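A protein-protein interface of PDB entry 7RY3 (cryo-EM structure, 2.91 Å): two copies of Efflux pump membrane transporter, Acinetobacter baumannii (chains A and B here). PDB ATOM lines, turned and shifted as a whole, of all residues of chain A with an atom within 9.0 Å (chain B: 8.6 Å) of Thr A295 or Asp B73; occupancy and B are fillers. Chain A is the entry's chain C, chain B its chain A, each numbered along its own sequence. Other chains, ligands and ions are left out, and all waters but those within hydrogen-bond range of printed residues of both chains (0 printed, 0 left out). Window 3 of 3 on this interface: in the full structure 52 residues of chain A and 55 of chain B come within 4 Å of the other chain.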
ATOM      1  N   PRO A  31       8.444   0.870 -28.413  1.00  0.00           N
ATOM      2  CA  PRO A  31       7.884   2.169 -28.782  1.00  0.00           C
ATOM      3  C   PRO A  31       8.960   3.188 -29.080  1.00  0.00           C
ATOM      4  O   PRO A  31      10.011   3.163 -28.452  1.00  0.00           O
ATOM      5  CB  PRO A  31       7.117   2.588 -27.524  1.00  0.00           C
ATOM      6  CG  PRO A  31       7.562   1.670 -26.437  1.00  0.00           C
ATOM      7  CD  PRO A  31       7.912   0.394 -27.128  1.00  0.00           C
ATOM      8  N   ILE A  32       8.718   4.064 -30.043  1.00  0.00           N
ATOM      9  CA  ILE A  32       9.670   5.121 -30.332  1.00  0.00           C
ATOM     10  C   ILE A  32       9.003   6.478 -30.234  1.00  0.00           C
ATOM     11  O   ILE A  32       7.897   6.650 -30.727  1.00  0.00           O
ATOM     12  CB  ILE A  32      10.313   4.954 -31.731  1.00  0.00           C
ATOM     13  CG1 ILE A  32      10.976   3.586 -31.865  1.00  0.00           C
ATOM     14  CG2 ILE A  32      11.323   6.049 -32.020  1.00  0.00           C
ATOM     15  CD1 ILE A  32      11.675   3.376 -33.189  1.00  0.00           C
ATOM     16  N   ALA A  33       9.670   7.439 -29.607  1.00  0.00           N
ATOM     17  CA  ALA A  33       9.141   8.800 -29.473  1.00  0.00           C
ATOM     18  C   ALA A  33      10.256   9.815 -29.384  1.00  0.00           C
ATOM     19  O   ALA A  33      11.407   9.456 -29.210  1.00  0.00           O
ATOM     20  CB  ALA A  33       8.270   8.906 -28.255  1.00  0.00           C
ATOM     21  N   THR A  37       7.277  11.937 -22.020  1.00  0.00           N
ATOM     22  CA  THR A  37       6.257  12.403 -21.052  1.00  0.00           C
ATOM     23  C   THR A  37       6.753  13.205 -19.854  1.00  0.00           C
ATOM     24  O   THR A  37       6.400  12.902 -18.725  1.00  0.00           O
ATOM     25  CB  THR A  37       5.285  11.296 -20.601  1.00  0.00           C
ATOM     26  OG1 THR A  37       6.007  10.217 -19.993  1.00  0.00           O
ATOM     27  CG2 THR A  37       4.490  10.769 -21.785  1.00  0.00           C
ATOM     28  N   ASP A  99      -2.171   9.534 -11.524  1.00  0.00           N
ATOM     29  CA  ASP A  99      -2.578   8.966 -12.798  1.00  0.00           C
ATOM     30  C   ASP A  99      -3.483   9.903 -13.523  1.00  0.00           C
ATOM     31  O   ASP A  99      -4.464  10.376 -12.970  1.00  0.00           O
ATOM     32  CB  ASP A  99      -3.314   7.650 -12.587  1.00  0.00           C
ATOM     33  CG  ASP A  99      -3.733   6.996 -13.888  1.00  0.00           C
ATOM     34  OD1 ASP A  99      -2.853   6.704 -14.724  1.00  0.00           O
ATOM     35  OD2 ASP A  99      -4.942   6.758 -14.071  1.00  0.00           O
ATOM     36  N   ASP A 101      -5.705   9.650 -16.118  1.00  0.00           N
ATOM     37  CA  ASP A 101      -7.087   9.270 -16.299  1.00  0.00           C
ATOM     38  C   ASP A 101      -7.910   9.437 -15.041  1.00  0.00           C
ATOM     39  O   ASP A 101      -9.049   9.874 -15.103  1.00  0.00           O
ATOM     40  CB  ASP A 101      -7.141   7.810 -16.690  1.00  0.00           C
ATOM     41  CG  ASP A 101      -6.259   7.486 -17.874  1.00  0.00           C
ATOM     42  OD1 ASP A 101      -6.140   8.329 -18.783  1.00  0.00           O
ATOM     43  OD2 ASP A 101      -5.694   6.374 -17.905  1.00  0.00           O
ATOM     44  N   LYS A 131      -7.267  16.669 -20.987  1.00  0.00           N
ATOM     45  CA  LYS A 131      -6.049  16.472 -20.203  1.00  0.00           C
ATOM     46  C   LYS A 131      -4.759  16.609 -20.978  1.00  0.00           C
ATOM     47  O   LYS A 131      -4.747  16.478 -22.189  1.00  0.00           O
ATOM     48  CB  LYS A 131      -6.081  15.150 -19.447  1.00  0.00           C
ATOM     49  CG  LYS A 131      -6.050  13.886 -20.275  1.00  0.00           C
ATOM     50  CD  LYS A 131      -5.877  12.698 -19.345  1.00  0.00           C
ATOM     51  CE  LYS A 131      -6.134  11.384 -20.046  1.00  0.00           C
ATOM     52  NZ  LYS A 131      -5.193  11.189 -21.178  1.00  0.00           N
ATOM     53  N   GLY A 133      -0.895  15.717 -22.288  1.00  0.00           N
ATOM     54  CA  GLY A 133      -0.474  14.474 -22.883  1.00  0.00           C
ATOM     55  C   GLY A 133       0.553  14.540 -23.966  1.00  0.00           C
ATOM     56  O   GLY A 133       1.570  15.211 -23.817  1.00  0.00           O
ATOM     57  N   ALA A 134       0.306  13.837 -25.058  1.00  0.00           N
ATOM     58  CA  ALA A 134       1.292  13.766 -26.115  1.00  0.00           C
ATOM     59  C   ALA A 134       1.444  15.036 -26.855  1.00  0.00           C
ATOM     60  O   ALA A 134       0.488  15.791 -26.991  1.00  0.00           O
ATOM     61  CB  ALA A 134       0.968  12.640 -27.082  1.00  0.00           C
ATOM     62  N   ALA A 170      -3.552   3.619 -37.998  1.00  0.00           N
ATOM     63  CA  ALA A 170      -2.853   3.068 -36.858  1.00  0.00           C
ATOM     64  C   ALA A 170      -1.803   3.907 -36.193  1.00  0.00           C
ATOM     65  O   ALA A 170      -0.918   4.425 -36.851  1.00  0.00           O
ATOM     66  CB  ALA A 170      -2.242   1.749 -37.272  1.00  0.00           C
ATOM     67  N   GLY A 171      -1.883   4.011 -34.879  1.00  0.00           N
ATOM     68  CA  GLY A 171      -0.995   4.850 -34.114  1.00  0.00           C
ATOM     69  C   GLY A 171      -1.490   6.237 -33.808  1.00  0.00           C
ATOM     70  O   GLY A 171      -0.815   6.984 -33.117  1.00  0.00           O
ATOM     71  N   VAL A 172      -2.666   6.590 -34.302  1.00  0.00           N
ATOM     72  CA  VAL A 172      -3.147   7.931 -34.105  1.00  0.00           C
ATOM     73  C   VAL A 172      -4.068   8.036 -32.909  1.00  0.00           C
ATOM     74  O   VAL A 172      -5.238   7.662 -32.976  1.00  0.00           O
ATOM     75  CB  VAL A 172      -3.837   8.459 -35.366  1.00  0.00           C
ATOM     76  CG1 VAL A 172      -4.324   9.877 -35.136  1.00  0.00           C
ATOM     77  CG2 VAL A 172      -2.890   8.411 -36.550  1.00  0.00           C
ATOM     78  N   GLY A 173      -3.541   8.525 -31.799  1.00  0.00           N
ATOM     79  CA  GLY A 173      -4.352   8.701 -30.620  1.00  0.00           C
ATOM     80  C   GLY A 173      -5.388   9.780 -30.728  1.00  0.00           C
ATOM     81  O   GLY A 173      -6.501   9.629 -30.243  1.00  0.00           O
ATOM     82  N   GLU A 174      -5.027  10.880 -31.369  1.00  0.00           N
ATOM     83  CA  GLU A 174      -5.956  11.987 -31.465  1.00  0.00           C
ATOM     84  C   GLU A 174      -5.804  12.817 -32.714  1.00  0.00           C
ATOM     85  O   GLU A 174      -4.695  13.060 -33.156  1.00  0.00           O
ATOM     86  CB  GLU A 174      -5.803  12.880 -30.241  1.00  0.00           C
ATOM     87  CG  GLU A 174      -6.605  14.170 -30.295  1.00  0.00           C
ATOM     88  CD  GLU A 174      -6.490  14.974 -29.018  1.00  0.00           C
ATOM     89  OE1 GLU A 174      -5.890  14.466 -28.048  1.00  0.00           O
ATOM     90  OE2 GLU A 174      -6.996  16.114 -28.985  1.00  0.00           O
ATOM     91  N   LYS A 292      -1.845  13.659 -33.031  1.00  0.00           N
ATOM     92  CA  LYS A 292      -1.187  13.284 -31.785  1.00  0.00           C
ATOM     93  C   LYS A 292      -0.994  11.782 -31.823  1.00  0.00           C
ATOM     94  O   LYS A 292      -1.929  11.055 -32.105  1.00  0.00           O
ATOM     95  CB  LYS A 292      -1.989  13.708 -30.572  1.00  0.00           C
ATOM     96  CG  LYS A 292      -2.766  14.986 -30.779  1.00  0.00           C
ATOM     97  CD  LYS A 292      -3.179  15.596 -29.458  1.00  0.00           C
ATOM     98  CE  LYS A 292      -1.985  16.132 -28.703  1.00  0.00           C
ATOM     99  NZ  LYS A 292      -2.386  16.829 -27.451  1.00  0.00           N
ATOM    100  N   ILE A 293       0.207  11.307 -31.563  1.00  0.00           N
ATOM    101  CA  ILE A 293       0.480   9.880 -31.575  1.00  0.00           C
ATOM    102  C   ILE A 293      -0.195   9.169 -30.398  1.00  0.00           C
ATOM    103  O   ILE A 293      -0.510   9.789 -29.392  1.00  0.00           O
ATOM    104  CB  ILE A 293       2.012   9.631 -31.626  1.00  0.00           C
ATOM    105  CG1 ILE A 293       2.355   8.190 -31.974  1.00  0.00           C
ATOM    106  CG2 ILE A 293       2.675  10.025 -30.314  1.00  0.00           C
ATOM    107  CD1 ILE A 293       3.700   7.787 -31.424  1.00  0.00           C
ATOM    108  N   ALA A 294      -0.446   7.868 -30.530  1.00  0.00           N
ATOM    109  CA  ALA A 294      -1.130   7.095 -29.489  1.00  0.00           C
ATOM    110  C   ALA A 294      -0.127   6.470 -28.578  1.00  0.00           C
ATOM    111  O   ALA A 294       1.054   6.422 -28.879  1.00  0.00           O
ATOM    112  CB  ALA A 294      -1.991   6.020 -30.109  1.00  0.00           C
ATOM    113  N   THR A 295      -0.602   6.001 -27.434  1.00  0.00           N
ATOM    114  CA  THR A 295       0.287   5.452 -26.422  1.00  0.00           C
ATOM    115  C   THR A 295       1.015   4.217 -26.914  1.00  0.00           C
ATOM    116  O   THR A 295       0.425   3.373 -27.588  1.00  0.00           O
ATOM    117  CB  THR A 295      -0.504   5.086 -25.164  1.00  0.00           C
ATOM    118  OG1 THR A 295      -1.488   6.096 -24.910  1.00  0.00           O
ATOM    119  CG2 THR A 295       0.414   4.968 -23.956  1.00  0.00           C
ATOM    120  N   GLY A 296       2.295   4.073 -26.594  1.00  0.00           N
ATOM    121  CA  GLY A 296       2.934   2.816 -26.941  1.00  0.00           C
ATOM    122  C   GLY A 296       3.025   2.714 -28.428  1.00  0.00           C
ATOM    123  O   GLY A 296       2.615   1.705 -28.982  1.00  0.00           O
ATOM    124  N   ALA A 297       3.569   3.709 -29.100  1.00  0.00           N
ATOM    125  CA  ALA A 297       3.543   3.687 -30.557  1.00  0.00           C
ATOM    126  C   ALA A 297       4.818   4.150 -31.195  1.00  0.00           C
ATOM    127  O   ALA A 297       5.605   4.840 -30.563  1.00  0.00           O
ATOM    128  CB  ALA A 297       2.373   4.492 -31.062  1.00  0.00           C
ATOM    129  N   ASN A 298       5.038   3.790 -32.456  1.00  0.00           N
ATOM    130  CA  ASN A 298       6.208   4.302 -33.143  1.00  0.00           C
ATOM    131  C   ASN A 298       5.698   5.422 -33.975  1.00  0.00           C
ATOM    132  O   ASN A 298       4.801   5.242 -34.776  1.00  0.00           O
ATOM    133  CB  ASN A 298       6.827   3.233 -34.048  1.00  0.00           C
ATOM    134  CG  ASN A 298       8.114   3.691 -34.701  1.00  0.00           C
ATOM    135  OD1 ASN A 298       8.644   4.754 -34.389  1.00  0.00           O
ATOM    136  ND2 ASN A 298       8.629   2.881 -35.608  1.00  0.00           N
ATOM    137  N   ALA A 299       6.235   6.605 -33.729  1.00  0.00           N
ATOM    138  CA  ALA A 299       5.836   7.783 -34.465  1.00  0.00           C
ATOM    139  C   ALA A 299       6.243   7.697 -35.890  1.00  0.00           C
ATOM    140  O   ALA A 299       5.540   8.164 -36.762  1.00  0.00           O
ATOM    141  CB  ALA A 299       6.435   9.014 -33.816  1.00  0.00           C
ATOM    142  N   THR A 302       3.682   5.610 -37.516  1.00  0.00           N
ATOM    143  CA  THR A 302       2.404   6.287 -37.576  1.00  0.00           C
ATOM    144  C   THR A 302       2.455   7.338 -38.667  1.00  0.00           C
ATOM    145  O   THR A 302       1.514   7.479 -39.434  1.00  0.00           O
ATOM    146  CB  THR A 302       2.069   6.949 -36.216  1.00  0.00           C
ATOM    147  OG1 THR A 302       1.939   5.942 -35.213  1.00  0.00           O
ATOM    148  CG2 THR A 302       0.785   7.735 -36.287  1.00  0.00           C
ATOM    149  N   PRO B  41     -12.270  -7.582 -21.607  1.00  0.00           N
ATOM    150  CA  PRO B  41     -13.140  -6.501 -21.143  1.00  0.00           C
ATOM    151  C   PRO B  41     -13.966  -5.865 -22.245  1.00  0.00           C
ATOM    152  O   PRO B  41     -13.494  -5.718 -23.367  1.00  0.00           O
ATOM    153  CB  PRO B  41     -12.151  -5.480 -20.568  1.00  0.00           C
ATOM    154  CG  PRO B  41     -10.822  -5.839 -21.135  1.00  0.00           C
ATOM    155  CD  PRO B  41     -10.846  -7.315 -21.354  1.00  0.00           C
ATOM    156  N   MET B  69     -13.436   7.332 -29.920  1.00  0.00           N
ATOM    157  CA  MET B  69     -12.887   6.202 -29.203  1.00  0.00           C
ATOM    158  C   MET B  69     -11.835   5.395 -29.920  1.00  0.00           C
ATOM    159  O   MET B  69     -11.345   4.411 -29.387  1.00  0.00           O
ATOM    160  CB  MET B  69     -14.031   5.271 -28.801  1.00  0.00           C
ATOM    161  CG  MET B  69     -15.352   5.955 -28.479  1.00  0.00           C
ATOM    162  SD  MET B  69     -15.335   6.991 -27.005  1.00  0.00           S
ATOM    163  CE  MET B  69     -14.499   5.889 -25.903  1.00  0.00           C
ATOM    164  N   ASN B  70     -11.455   5.820 -31.111  1.00  0.00           N
ATOM    165  CA  ASN B  70     -10.444   5.115 -31.915  1.00  0.00           C
ATOM    166  C   ASN B  70      -9.040   4.985 -31.294  1.00  0.00           C
ATOM    167  O   ASN B  70      -8.381   3.975 -31.502  1.00  0.00           O
ATOM    168  CB  ASN B  70     -10.377   5.706 -33.330  1.00  0.00           C
ATOM    169  CG  ASN B  70     -11.600   5.396 -34.149  1.00  0.00           C
ATOM    170  OD1 ASN B  70     -12.340   4.466 -33.847  1.00  0.00           O
ATOM    171  ND2 ASN B  70     -11.815   6.167 -35.202  1.00  0.00           N
ATOM    172  N   GLY B  71      -8.581   5.984 -30.552  1.00  0.00           N
ATOM    173  CA  GLY B  71      -7.247   5.980 -29.954  1.00  0.00           C
ATOM    174  C   GLY B  71      -7.110   5.343 -28.584  1.00  0.00           C
ATOM    175  O   GLY B  71      -6.045   5.396 -27.995  1.00  0.00           O
ATOM    176  N   LEU B  72      -8.176   4.744 -28.069  1.00  0.00           N
ATOM    177  CA  LEU B  72      -8.157   4.130 -26.745  1.00  0.00           C
ATOM    178  C   LEU B  72      -7.168   3.001 -26.618  1.00  0.00           C
ATOM    179  O   LEU B  72      -7.025   2.192 -27.527  1.00  0.00           O
ATOM    180  CB  LEU B  72      -9.528   3.547 -26.413  1.00  0.00           C
ATOM    181  CG  LEU B  72     -10.711   4.396 -25.975  1.00  0.00           C
ATOM    182  CD1 LEU B  72     -11.938   3.506 -26.029  1.00  0.00           C
ATOM    183  CD2 LEU B  72     -10.493   4.926 -24.571  1.00  0.00           C
ATOM    184  N   ASP B  73      -6.481   2.942 -25.483  1.00  0.00           N
ATOM    185  CA  ASP B  73      -5.501   1.910 -25.290  1.00  0.00           C
ATOM    186  C   ASP B  73      -6.028   0.505 -25.174  1.00  0.00           C
ATOM    187  O   ASP B  73      -6.927   0.239 -24.391  1.00  0.00           O
ATOM    188  CB  ASP B  73      -4.676   2.244 -24.058  1.00  0.00           C
ATOM    189  CG  ASP B  73      -3.994   3.591 -24.163  1.00  0.00           C
ATOM    190  OD1 ASP B  73      -3.896   4.126 -25.288  1.00  0.00           O
ATOM    191  OD2 ASP B  73      -3.546   4.113 -23.121  1.00  0.00           O
ATOM    192  N   GLY B  74      -5.442  -0.406 -25.939  1.00  0.00           N
ATOM    193  CA  GLY B  74      -5.867  -1.784 -25.932  1.00  0.00           C
ATOM    194  C   GLY B  74      -7.148  -2.171 -26.606  1.00  0.00           C
ATOM    195  O   GLY B  74      -7.740  -3.142 -26.199  1.00  0.00           O
ATOM    196  N   LEU B  75      -7.568  -1.471 -27.637  1.00  0.00           N
ATOM    197  CA  LEU B  75      -8.864  -1.746 -28.220  1.00  0.00           C
ATOM    198  C   LEU B  75      -8.768  -2.737 -29.350  1.00  0.00           C
ATOM    199  O   LEU B  75      -8.252  -2.419 -30.406  1.00  0.00           O
ATOM    200  CB  LEU B  75      -9.443  -0.441 -28.755  1.00  0.00           C
ATOM    201  CG  LEU B  75     -10.823  -0.372 -29.398  1.00  0.00           C
ATOM    202  CD1 LEU B  75     -11.908  -0.664 -28.376  1.00  0.00           C
ATOM    203  CD2 LEU B  75     -10.970   1.032 -29.947  1.00  0.00           C
ATOM    204  N   ARG B  76      -9.306  -3.928 -29.150  1.00  0.00           N
ATOM    205  CA  ARG B  76      -9.261  -4.947 -30.183  1.00  0.00           C
ATOM    206  C   ARG B  76     -10.183  -4.635 -31.374  1.00  0.00           C
ATOM    207  O   ARG B  76      -9.709  -4.590 -32.501  1.00  0.00           O
ATOM    208  CB  ARG B  76      -9.500  -6.339 -29.583  1.00  0.00           C
ATOM    209  CG  ARG B  76      -8.777  -7.452 -30.314  1.00  0.00           C
ATOM    210  CD  ARG B  76      -8.549  -8.633 -29.393  1.00  0.00           C
ATOM    211  NE  ARG B  76      -9.731  -9.473 -29.280  1.00  0.00           N
ATOM    212  CZ  ARG B  76      -9.840 -10.674 -29.827  1.00  0.00           C
ATOM    213  NH1 ARG B  76      -8.831 -11.182 -30.512  1.00  0.00           N
ATOM    214  NH2 ARG B  76     -10.955 -11.370 -29.680  1.00  0.00           N
ATOM    215  N   ASN B  93     -14.442  -3.612 -27.670  1.00  0.00           N
ATOM    216  CA  ASN B  93     -13.779  -4.800 -27.171  1.00  0.00           C
ATOM    217  C   ASN B  93     -12.315  -4.562 -26.982  1.00  0.00           C
ATOM    218  O   ASN B  93     -11.634  -4.087 -27.872  1.00  0.00           O
ATOM    219  CB  ASN B  93     -14.063  -6.004 -28.060  1.00  0.00           C
ATOM    220  CG  ASN B  93     -15.506  -6.456 -27.987  1.00  0.00           C
ATOM    221  OD1 ASN B  93     -15.813  -7.466 -27.363  1.00  0.00           O
ATOM    222  ND2 ASN B  93     -16.398  -5.712 -28.627  1.00  0.00           N
ATOM    223  N   PHE B  94     -11.825  -4.882 -25.803  1.00  0.00           N
ATOM    224  CA  PHE B  94     -10.445  -4.597 -25.486  1.00  0.00           C
ATOM    225  C   PHE B  94      -9.627  -5.859 -25.419  1.00  0.00           C
ATOM    226  O   PHE B  94     -10.161  -6.945 -25.265  1.00  0.00           O
ATOM    227  CB  PHE B  94     -10.336  -3.811 -24.173  1.00  0.00           C
ATOM    228  CG  PHE B  94     -10.967  -2.457 -24.211  1.00  0.00           C
ATOM    229  CD1 PHE B  94     -12.297  -2.286 -23.875  1.00  0.00           C
ATOM    230  CD2 PHE B  94     -10.218  -1.348 -24.551  1.00  0.00           C
ATOM    231  CE1 PHE B  94     -12.874  -1.035 -23.897  1.00  0.00           C
ATOM    232  CE2 PHE B  94     -10.788  -0.093 -24.577  1.00  0.00           C
ATOM    233  CZ  PHE B  94     -12.117   0.064 -24.247  1.00  0.00           C
ATOM    234  N   GLU B  95      -8.328  -5.736 -25.499  1.00  0.00           N
ATOM    235  CA  GLU B  95      -7.463  -6.889 -25.479  1.00  0.00           C
ATOM    236  C   GLU B  95      -7.170  -7.439 -24.105  1.00  0.00           C
ATOM    237  O   GLU B  95      -7.211  -6.725 -23.129  1.00  0.00           O
ATOM    238  CB  GLU B  95      -6.158  -6.505 -26.165  1.00  0.00           C
ATOM    239  CG  GLU B  95      -6.335  -6.033 -27.591  1.00  0.00           C
ATOM    240  CD  GLU B  95      -5.266  -5.055 -28.021  1.00  0.00           C
ATOM    241  OE1 GLU B  95      -4.330  -4.811 -27.232  1.00  0.00           O
ATOM    242  OE2 GLU B  95      -5.369  -4.522 -29.146  1.00  0.00           O
ATOM    243  N   GLY B  97      -5.639  -8.398 -20.861  1.00  0.00           N
ATOM    244  CA  GLY B  97      -4.594  -7.646 -20.244  1.00  0.00           C
ATOM    245  C   GLY B  97      -5.092  -6.316 -19.786  1.00  0.00           C
ATOM    246  O   GLY B  97      -4.504  -5.696 -18.903  1.00  0.00           O
ATOM    247  N   VAL B  98      -6.183  -5.866 -20.378  1.00  0.00           N
ATOM    248  CA  VAL B  98      -6.662  -4.535 -20.098  1.00  0.00           C
ATOM    249  C   VAL B  98      -7.538  -4.662 -18.876  1.00  0.00           C
ATOM    250  O   VAL B  98      -8.416  -5.510 -18.835  1.00  0.00           O
ATOM    251  CB  VAL B  98      -7.416  -3.933 -21.299  1.00  0.00           C
ATOM    252  CG1 VAL B  98      -8.018  -2.587 -20.937  1.00  0.00           C
ATOM    253  CG2 VAL B  98      -6.490  -3.796 -22.494  1.00  0.00           C
ATOM    254  N   ASP B  99      -7.278  -3.852 -17.860  1.00  0.00           N
ATOM    255  CA  ASP B  99      -8.135  -3.842 -16.681  1.00  0.00           C
ATOM    256  C   ASP B  99      -9.484  -3.275 -17.029  1.00  0.00           C
ATOM    257  O   ASP B  99      -9.570  -2.217 -17.636  1.00  0.00           O
ATOM    258  CB  ASP B  99      -7.519  -3.017 -15.566  1.00  0.00           C
ATOM    259  CG  ASP B  99      -8.239  -3.186 -14.249  1.00  0.00           C
ATOM    260  OD1 ASP B  99      -8.184  -4.294 -13.679  1.00  0.00           O
ATOM    261  OD2 ASP B  99      -8.853  -2.212 -13.774  1.00  0.00           O
ATOM    262  N   ILE B 102     -10.336   0.264 -15.438  1.00  0.00           N
ATOM    263  CA  ILE B 102      -9.595   1.411 -15.893  1.00  0.00           C
ATOM    264  C   ILE B 102     -10.058   1.723 -17.282  1.00  0.00           C
ATOM    265  O   ILE B 102     -10.160   2.888 -17.638  1.00  0.00           O
ATOM    266  CB  ILE B 102      -8.089   1.089 -15.867  1.00  0.00           C
ATOM    267  CG1 ILE B 102      -7.633   0.841 -14.432  1.00  0.00           C
ATOM    268  CG2 ILE B 102      -7.273   2.214 -16.482  1.00  0.00           C
ATOM    269  CD1 ILE B 102      -7.915   1.998 -13.499  1.00  0.00           C
ATOM    270  N   ALA B 103     -10.399   0.709 -18.069  1.00  0.00           N
ATOM    271  CA  ALA B 103     -10.941   0.932 -19.413  1.00  0.00           C
ATOM    272  C   ALA B 103     -12.234   1.709 -19.382  1.00  0.00           C
ATOM    273  O   ALA B 103     -12.526   2.461 -20.296  1.00  0.00           O
ATOM    274  CB  ALA B 103     -11.134  -0.389 -20.135  1.00  0.00           C
ATOM    275  N   GLN B 106     -11.510   5.339 -18.931  1.00  0.00           N
ATOM    276  CA  GLN B 106     -11.015   5.891 -20.183  1.00  0.00           C
ATOM    277  C   GLN B 106     -12.056   6.240 -21.233  1.00  0.00           C
ATOM    278  O   GLN B 106     -11.946   7.266 -21.884  1.00  0.00           O
ATOM    279  CB  GLN B 106      -9.969   4.956 -20.758  1.00  0.00           C
ATOM    280  CG  GLN B 106      -8.695   4.937 -19.941  1.00  0.00           C
ATOM    281  CD  GLN B 106      -7.643   4.026 -20.521  1.00  0.00           C
ATOM    282  OE1 GLN B 106      -7.774   3.551 -21.645  1.00  0.00           O
ATOM    283  NE2 GLN B 106      -6.584   3.782 -19.759  1.00  0.00           N
ATOM    284  N   VAL B 107     -13.054   5.390 -21.418  1.00  0.00           N
ATOM    285  CA  VAL B 107     -14.120   5.620 -22.391  1.00  0.00           C
ATOM    286  C   VAL B 107     -14.864   6.848 -21.965  1.00  0.00           C
ATOM    287  O   VAL B 107     -15.171   7.699 -22.779  1.00  0.00           O
ATOM    288  CB  VAL B 107     -15.045   4.383 -22.492  1.00  0.00           C
ATOM    289  CG1 VAL B 107     -16.380   4.707 -23.137  1.00  0.00           C
ATOM    290  CG2 VAL B 107     -14.342   3.228 -23.176  1.00  0.00           C
ATOM    291  N   LYS B 110     -13.071   9.978 -22.811  1.00  0.00           N
ATOM    292  CA  LYS B 110     -13.209  10.285 -24.230  1.00  0.00           C
ATOM    293  C   LYS B 110     -14.572  10.873 -24.565  1.00  0.00           C
ATOM    294  O   LYS B 110     -14.677  11.757 -25.404  1.00  0.00           O
ATOM    295  CB  LYS B 110     -12.878   9.053 -25.068  1.00  0.00           C
ATOM    296  CG  LYS B 110     -11.402   8.759 -25.177  1.00  0.00           C
ATOM    297  CD  LYS B 110     -10.678   9.912 -25.841  1.00  0.00           C
ATOM    298  CE  LYS B 110      -9.191   9.624 -25.942  1.00  0.00           C
ATOM    299  NZ  LYS B 110      -8.599   9.360 -24.602  1.00  0.00           N
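The side-chain carboxylate (OD1) of Asp B73 sits at hydrogen-bond distance from the side-chain hydroxyl (OG1) of Thr A295 (3.1 Å). NE2 of Gln B106 sits at hydrogen-bond distance from OD2 of Asp A101 (3.3 Å).
OD1 of Asp A101 lies within salt-bridge range of NZ of Lys A131 (3.8 Å). The backbone NH (N) of Gly A173 lies within hydrogen-bond range of the backbone carbonyl oxygen (O) of Lys A292 (3.0 Å).
O of Val A172 touches CA of Gly B71, 3.9997 Å away. O of Gly A173 touches CA of Gly B71 (3.7 Å).
Of chain B, only Asp B73 comes within 4 Å of Thr A295. Of the printed residues of chain A, Asp B73 touches Thr A295 (3.1 Å). Ala A294 touches none of the printed residues of chain B. No residue of chain B comes within 4 Å of Gly A296. Gly B74 touches none of the printed residues of chain A. Of the printed residues of chain A, Gly B71 touches Val A172 and Gly A173. Printed residues of chain B within 4 Å of Gly A173: Gly B71. Of the printed residues of chain B, Val A172 touches Gly B71 (3.9997 Å). Printed residues of chain B within 4 Å of Asp A101: Gln B106. Of the printed residues of chain A, Gln B106 touches Asp A101. Asn A298 touches none of the printed residues of chain B. Asp A99 touches none of the printed residues of chain B. The nearest residue of chain B that does not touch Thr A295 is Gly B71 (5.5 Å). The nearest printed residue of chain B that does not touch Asp A101 is Ile B102 (4.7 Å).
Printed residues of chain B that touch a printed residue of chain A: Gly B71, Asp B73 and Gln B106. Along chain B the printed residues that touch a printed residue of chain A span positions 71 to 106. Among the printed residues, 4 pairs touch across the chains.
Position printed for both chains: 99. Of the 4 pairs that touch across the chains among the printed residues, none has its exchanged pair printed and touching as well.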
